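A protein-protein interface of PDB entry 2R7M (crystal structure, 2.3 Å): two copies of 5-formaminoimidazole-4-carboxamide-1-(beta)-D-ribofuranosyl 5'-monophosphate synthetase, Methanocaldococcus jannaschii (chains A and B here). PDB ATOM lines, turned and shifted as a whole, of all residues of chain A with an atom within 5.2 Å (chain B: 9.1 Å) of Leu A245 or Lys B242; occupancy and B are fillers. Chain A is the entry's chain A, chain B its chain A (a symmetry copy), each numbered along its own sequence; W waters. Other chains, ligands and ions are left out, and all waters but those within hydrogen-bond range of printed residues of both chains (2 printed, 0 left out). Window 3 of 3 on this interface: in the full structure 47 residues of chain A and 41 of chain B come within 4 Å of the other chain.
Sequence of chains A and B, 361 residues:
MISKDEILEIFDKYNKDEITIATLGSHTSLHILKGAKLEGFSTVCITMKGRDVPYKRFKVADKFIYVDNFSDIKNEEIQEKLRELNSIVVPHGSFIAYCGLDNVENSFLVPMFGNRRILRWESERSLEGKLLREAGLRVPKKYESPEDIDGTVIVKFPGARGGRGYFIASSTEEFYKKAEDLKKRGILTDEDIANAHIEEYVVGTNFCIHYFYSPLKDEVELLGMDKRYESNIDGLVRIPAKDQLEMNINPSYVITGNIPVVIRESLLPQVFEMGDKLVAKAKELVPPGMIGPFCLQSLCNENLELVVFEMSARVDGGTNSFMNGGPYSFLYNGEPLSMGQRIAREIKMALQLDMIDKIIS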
ATOM      1  N   PRO A 240       8.251 -18.648  24.317  1.00  0.00           N
ATOM      2  CA  PRO A 240       9.080 -18.736  25.533  1.00  0.00           C
ATOM      3  C   PRO A 240       9.858 -17.438  25.840  1.00  0.00           C
ATOM      4  O   PRO A 240      10.278 -16.734  24.932  1.00  0.00           O
ATOM      5  CB  PRO A 240      10.033 -19.889  25.227  1.00  0.00           C
ATOM      6  CG  PRO A 240       9.284 -20.738  24.199  1.00  0.00           C
ATOM      7  CD  PRO A 240       8.527 -19.743  23.367  1.00  0.00           C
ATOM      8  N   ALA A 241      10.011 -17.131  27.123  1.00  0.00           N
ATOM      9  CA  ALA A 241      10.643 -15.892  27.579  1.00  0.00           C
ATOM     10  C   ALA A 241      12.013 -15.619  26.926  1.00  0.00           C
ATOM     11  O   ALA A 241      12.286 -14.500  26.476  1.00  0.00           O
ATOM     12  CB  ALA A 241      10.754 -15.897  29.105  1.00  0.00           C
ATOM     13  N   LYS A 242      12.855 -16.647  26.855  1.00  0.00           N
ATOM     14  CA  LYS A 242      14.181 -16.532  26.229  1.00  0.00           C
ATOM     15  C   LYS A 242      14.111 -16.066  24.785  1.00  0.00           C
ATOM     16  O   LYS A 242      14.903 -15.234  24.349  1.00  0.00           O
ATOM     17  CB  LYS A 242      14.924 -17.870  26.291  1.00  0.00           C
ATOM     18  CG  LYS A 242      15.537 -18.169  27.652  1.00  0.00           C
ATOM     19  CD  LYS A 242      15.772 -19.655  27.836  1.00  0.00           C
ATOM     20  CE  LYS A 242      16.222 -19.969  29.253  1.00  0.00           C
ATOM     21  NZ  LYS A 242      17.543 -19.354  29.552  1.00  0.00           N
ATOM     22  N   ASP A 243      13.166 -16.617  24.038  1.00  0.00           N
ATOM     23  CA  ASP A 243      12.984 -16.235  22.643  1.00  0.00           C
ATOM     24  C   ASP A 243      12.355 -14.858  22.483  1.00  0.00           C
ATOM     25  O   ASP A 243      12.708 -14.121  21.572  1.00  0.00           O
ATOM     26  CB  ASP A 243      12.170 -17.296  21.912  1.00  0.00           C
ATOM     27  CG  ASP A 243      12.874 -18.620  21.873  1.00  0.00           C
ATOM     28  OD1 ASP A 243      13.960 -18.681  21.252  1.00  0.00           O
ATOM     29  OD2 ASP A 243      12.356 -19.593  22.465  1.00  0.00           O
ATOM     30  N   GLN A 244      11.415 -14.509  23.358  1.00  0.00           N
ATOM     31  CA  GLN A 244      10.816 -13.171  23.319  1.00  0.00           C
ATOM     32  C   GLN A 244      11.870 -12.065  23.449  1.00  0.00           C
ATOM     33  O   GLN A 244      11.750 -11.012  22.834  1.00  0.00           O
ATOM     34  CB  GLN A 244       9.809 -13.006  24.453  1.00  0.00           C
ATOM     35  CG  GLN A 244       8.417 -13.518  24.178  1.00  0.00           C
ATOM     36  CD  GLN A 244       7.484 -13.199  25.319  1.00  0.00           C
ATOM     37  OE1 GLN A 244       7.323 -12.034  25.697  1.00  0.00           O
ATOM     38  NE2 GLN A 244       6.875 -14.231  25.895  1.00  0.00           N
ATOM     39  N   LEU A 245      12.879 -12.302  24.286  1.00  0.00           N
ATOM     40  CA  LEU A 245      13.938 -11.320  24.534  1.00  0.00           C
ATOM     41  C   LEU A 245      14.841 -11.142  23.321  1.00  0.00           C
ATOM     42  O   LEU A 245      15.443 -10.084  23.142  1.00  0.00           O
ATOM     43  CB  LEU A 245      14.775 -11.706  25.762  1.00  0.00           C
ATOM     44  CG  LEU A 245      14.011 -11.830  27.081  1.00  0.00           C
ATOM     45  CD1 LEU A 245      14.977 -12.023  28.230  1.00  0.00           C
ATOM     46  CD2 LEU A 245      13.115 -10.613  27.321  1.00  0.00           C
ATOM     47  N   GLU A 246      14.924 -12.177  22.492  1.00  0.00           N
ATOM     48  CA  GLU A 246      15.648 -12.105  21.228  1.00  0.00           C
ATOM     49  C   GLU A 246      14.854 -11.424  20.121  1.00  0.00           C
ATOM     50  O   GLU A 246      15.360 -11.247  19.017  1.00  0.00           O
ATOM     51  CB  GLU A 246      16.058 -13.502  20.769  1.00  0.00           C
ATOM     52  CG  GLU A 246      17.251 -14.043  21.522  1.00  0.00           C
ATOM     53  CD  GLU A 246      17.518 -15.493  21.217  1.00  0.00           C
ATOM     54  OE1 GLU A 246      16.587 -16.318  21.367  1.00  0.00           O
ATOM     55  OE2 GLU A 246      18.664 -15.810  20.835  1.00  0.00           O
ATOM     56  N   MET A 247      13.613 -11.040  20.412  1.00  0.00           N
ATOM     57  CA  MET A 247      12.759 -10.427  19.397  1.00  0.00           C
ATOM     58  C   MET A 247      12.572  -8.938  19.645  1.00  0.00           C
ATOM     59  O   MET A 247      12.613  -8.469  20.784  1.00  0.00           O
ATOM     60  CB  MET A 247      11.383 -11.102  19.360  1.00  0.00           C
ATOM     61  CG  MET A 247      11.410 -12.598  19.096  1.00  0.00           C
ATOM     62  SD  MET A 247       9.825 -13.379  19.491  1.00  0.00           S
ATOM     63  CE  MET A 247       8.823 -12.842  18.102  1.00  0.00           C
ATOM     64  N   ILE A 249       9.635  -6.996  19.288  1.00  0.00           N
ATOM     65  CA  ILE A 249       8.211  -7.128  19.013  1.00  0.00           C
ATOM     66  C   ILE A 249       7.379  -6.418  20.071  1.00  0.00           C
ATOM     67  O   ILE A 249       7.602  -6.595  21.265  1.00  0.00           O
ATOM     68  CB  ILE A 249       7.800  -8.627  18.911  1.00  0.00           C
ATOM     69  CG1 ILE A 249       6.336  -8.774  18.479  1.00  0.00           C
ATOM     70  CG2 ILE A 249       8.065  -9.355  20.226  1.00  0.00           C
ATOM     71  CD1 ILE A 249       5.942 -10.202  18.153  1.00  0.00           C
ATOM     72  N   ILE B 239       1.522 -10.980  30.468  1.00  0.00           N
ATOM     73  CA  ILE B 239       2.365  -9.791  30.288  1.00  0.00           C
ATOM     74  C   ILE B 239       3.607 -10.210  29.513  1.00  0.00           C
ATOM     75  O   ILE B 239       4.218 -11.236  29.834  1.00  0.00           O
ATOM     76  CB  ILE B 239       2.786  -9.187  31.659  1.00  0.00           C
ATOM     77  CG1 ILE B 239       1.565  -8.711  32.445  1.00  0.00           C
ATOM     78  CG2 ILE B 239       3.770  -8.016  31.471  1.00  0.00           C
ATOM     79  CD1 ILE B 239       1.853  -8.415  33.926  1.00  0.00           C
ATOM     80  N   PRO B 240       3.975  -9.448  28.467  1.00  0.00           N
ATOM     81  CA  PRO B 240       5.196  -9.783  27.711  1.00  0.00           C
ATOM     82  C   PRO B 240       6.452  -9.906  28.600  1.00  0.00           C
ATOM     83  O   PRO B 240       6.589  -9.199  29.588  1.00  0.00           O
ATOM     84  CB  PRO B 240       5.329  -8.621  26.728  1.00  0.00           C
ATOM     85  CG  PRO B 240       3.903  -8.093  26.568  1.00  0.00           C
ATOM     86  CD  PRO B 240       3.282  -8.262  27.925  1.00  0.00           C
ATOM     87  N   ALA B 241       7.338 -10.828  28.241  1.00  0.00           N
ATOM     88  CA  ALA B 241       8.536 -11.134  29.027  1.00  0.00           C
ATOM     89  C   ALA B 241       9.367  -9.889  29.397  1.00  0.00           C
ATOM     90  O   ALA B 241       9.782  -9.729  30.551  1.00  0.00           O
ATOM     91  CB  ALA B 241       9.392 -12.165  28.287  1.00  0.00           C
ATOM     92  N   LYS B 242       9.582  -9.005  28.426  1.00  0.00           N
ATOM     93  CA  LYS B 242      10.332  -7.761  28.652  1.00  0.00           C
ATOM     94  C   LYS B 242       9.727  -6.901  29.749  1.00  0.00           C
ATOM     95  O   LYS B 242      10.439  -6.341  30.580  1.00  0.00           O
ATOM     96  CB  LYS B 242      10.419  -6.941  27.360  1.00  0.00           C
ATOM     97  CG  LYS B 242      11.465  -7.452  26.380  1.00  0.00           C
ATOM     98  CD  LYS B 242      11.163  -6.994  24.967  1.00  0.00           C
ATOM     99  CE  LYS B 242      12.107  -7.642  23.966  1.00  0.00           C
ATOM    100  NZ  LYS B 242      13.515  -7.218  24.192  1.00  0.00           N
ATOM    101  N   ASP B 243       8.408  -6.787  29.742  1.00  0.00           N
ATOM    102  CA  ASP B 243       7.710  -6.008  30.757  1.00  0.00           C
ATOM    103  C   ASP B 243       7.676  -6.696  32.114  1.00  0.00           C
ATOM    104  O   ASP B 243       7.772  -6.038  33.141  1.00  0.00           O
ATOM    105  CB  ASP B 243       6.301  -5.670  30.281  1.00  0.00           C
ATOM    106  CG  ASP B 243       6.312  -4.807  29.054  1.00  0.00           C
ATOM    107  OD1 ASP B 243       6.811  -3.663  29.154  1.00  0.00           O
ATOM    108  OD2 ASP B 243       5.836  -5.267  27.992  1.00  0.00           O
ATOM    109  N   GLN B 244       7.529  -8.018  32.126  1.00  0.00           N
ATOM    110  CA  GLN B 244       7.565  -8.764  33.387  1.00  0.00           C
ATOM    111  C   GLN B 244       8.871  -8.532  34.157  1.00  0.00           C
ATOM    112  O   GLN B 244       8.875  -8.477  35.381  1.00  0.00           O
ATOM    113  CB  GLN B 244       7.427 -10.261  33.126  1.00  0.00           C
ATOM    114  CG  GLN B 244       6.017 -10.777  32.987  1.00  0.00           C
ATOM    115  CD  GLN B 244       5.998 -12.279  32.846  1.00  0.00           C
ATOM    116  OE1 GLN B 244       6.516 -13.000  33.705  1.00  0.00           O
ATOM    117  NE2 GLN B 244       5.421 -12.766  31.751  1.00  0.00           N
ATOM    118  N   LEU B 245       9.982  -8.435  33.425  1.00  0.00           N
ATOM    119  CA  LEU B 245      11.303  -8.247  34.030  1.00  0.00           C
ATOM    120  C   LEU B 245      11.454  -6.861  34.642  1.00  0.00           C
ATOM    121  O   LEU B 245      12.237  -6.672  35.572  1.00  0.00           O
ATOM    122  CB  LEU B 245      12.420  -8.496  33.006  1.00  0.00           C
ATOM    123  CG  LEU B 245      12.450  -9.887  32.374  1.00  0.00           C
ATOM    124  CD1 LEU B 245      13.702 -10.056  31.540  1.00  0.00           C
ATOM    125  CD2 LEU B 245      12.352 -10.983  33.437  1.00  0.00           C
ATOM    126  N   GLU B 246      10.698  -5.901  34.120  1.00  0.00           N
ATOM    127  CA  GLU B 246      10.645  -4.558  34.686  1.00  0.00           C
ATOM    128  C   GLU B 246       9.736  -4.458  35.904  1.00  0.00           C
ATOM    129  O   GLU B 246       9.635  -3.399  36.515  1.00  0.00           O
ATOM    130  CB  GLU B 246      10.188  -3.554  33.631  1.00  0.00           C
ATOM    131  CG  GLU B 246      11.279  -3.191  32.652  1.00  0.00           C
ATOM    132  CD  GLU B 246      10.769  -2.370  31.496  1.00  0.00           C
ATOM    133  OE1 GLU B 246       9.809  -2.814  30.826  1.00  0.00           O
ATOM    134  OE2 GLU B 246      11.337  -1.285  31.254  1.00  0.00           O
ATOM    135  N   MET B 247       9.075  -5.557  36.261  1.00  0.00           N
ATOM    136  CA  MET B 247       8.139  -5.541  37.384  1.00  0.00           C
ATOM    137  C   MET B 247       8.697  -6.281  38.589  1.00  0.00           C
ATOM    138  O   MET B 247       9.487  -7.218  38.456  1.00  0.00           O
ATOM    139  CB  MET B 247       6.799  -6.171  36.988  1.00  0.00           C
ATOM    140  CG  MET B 247       6.108  -5.516  35.805  1.00  0.00           C
ATOM    141  SD  MET B 247       4.784  -6.557  35.139  1.00  0.00           S
ATOM    142  CE  MET B 247       3.516  -6.340  36.391  1.00  0.00           C
HETATM  143  O   HOH W   1       8.749  -9.233  25.354  1.00  0.00           O
HETATM  144  O   HOH W   2       5.084 -13.417  28.294  1.00  0.00           O
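The backbone NH of Ala B241 is in hydrogen-bond range of the side-chain amide oxygen of Gln A244.
Among the printed residues, pairs that only touch across the chains: Ala A241 with Ala B241, Gln A244 with Pro B240, Gln A244 with Lys B242, Leu A245 with Lys B242 and Met A247 with Lys B242.
Of the printed residues of chain B, Gln A244 touches Pro B240 (3.7 Å), Ala B241 (2.8 Å) and Lys B242 (3.6 Å). Leu A245 touches just one residue of chain B: Lys B242. Printed residues of chain B within 4 Å of Met A247: Lys B242 (3.3 Å). Of the printed residues of chain A, Pro B240 touches Gln A244. Of chain A, only Gln A244, Leu A245 and Met A247 come within 4 Å of Lys B242. The nearest printed residue of chain A that does not touch Pro B240 is Ile A249 (6.3 Å).
Of the 9 printed residues of chain A, 4 touch a printed residue of chain B. Printed residues of chain A that touch a printed residue of chain B: Ala A241, Gln A244, Leu A245 and Met A247. Of the 9 printed residues of chain B, 3 touch a printed residue of chain A. Printed residues of chain B that touch a printed residue of chain A: Pro B240, Ala B241 and Lys B242. Among the printed residues, 6 pairs touch across the chains.
Ala A241 touches its own counterpart, Ala B241. Gln A244 touches Ala B241, but with the chains exchanged Ala A241 does not touch Gln B244 (6.7 Å). Gln A244 touches Lys B242, but with the chains exchanged Lys A242 does not touch Gln B244 (9.7 Å). Leu A245 touches Lys B242, but with the chains exchanged Lys A242 does not touch Leu B245 (8.1 Å).
Water W2 lies within hydrogen-bond range of O of Ile B239 (2.8 Å), NE2 of Gln A244 (3.1 Å) and N of Ala B241 (3.4 Å). Water W1 bridges the side-chain amide oxygen (OE1) of Gln A244 (3.2 Å) and the backbone NH (N) of Lys B242 (3.2 Å).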
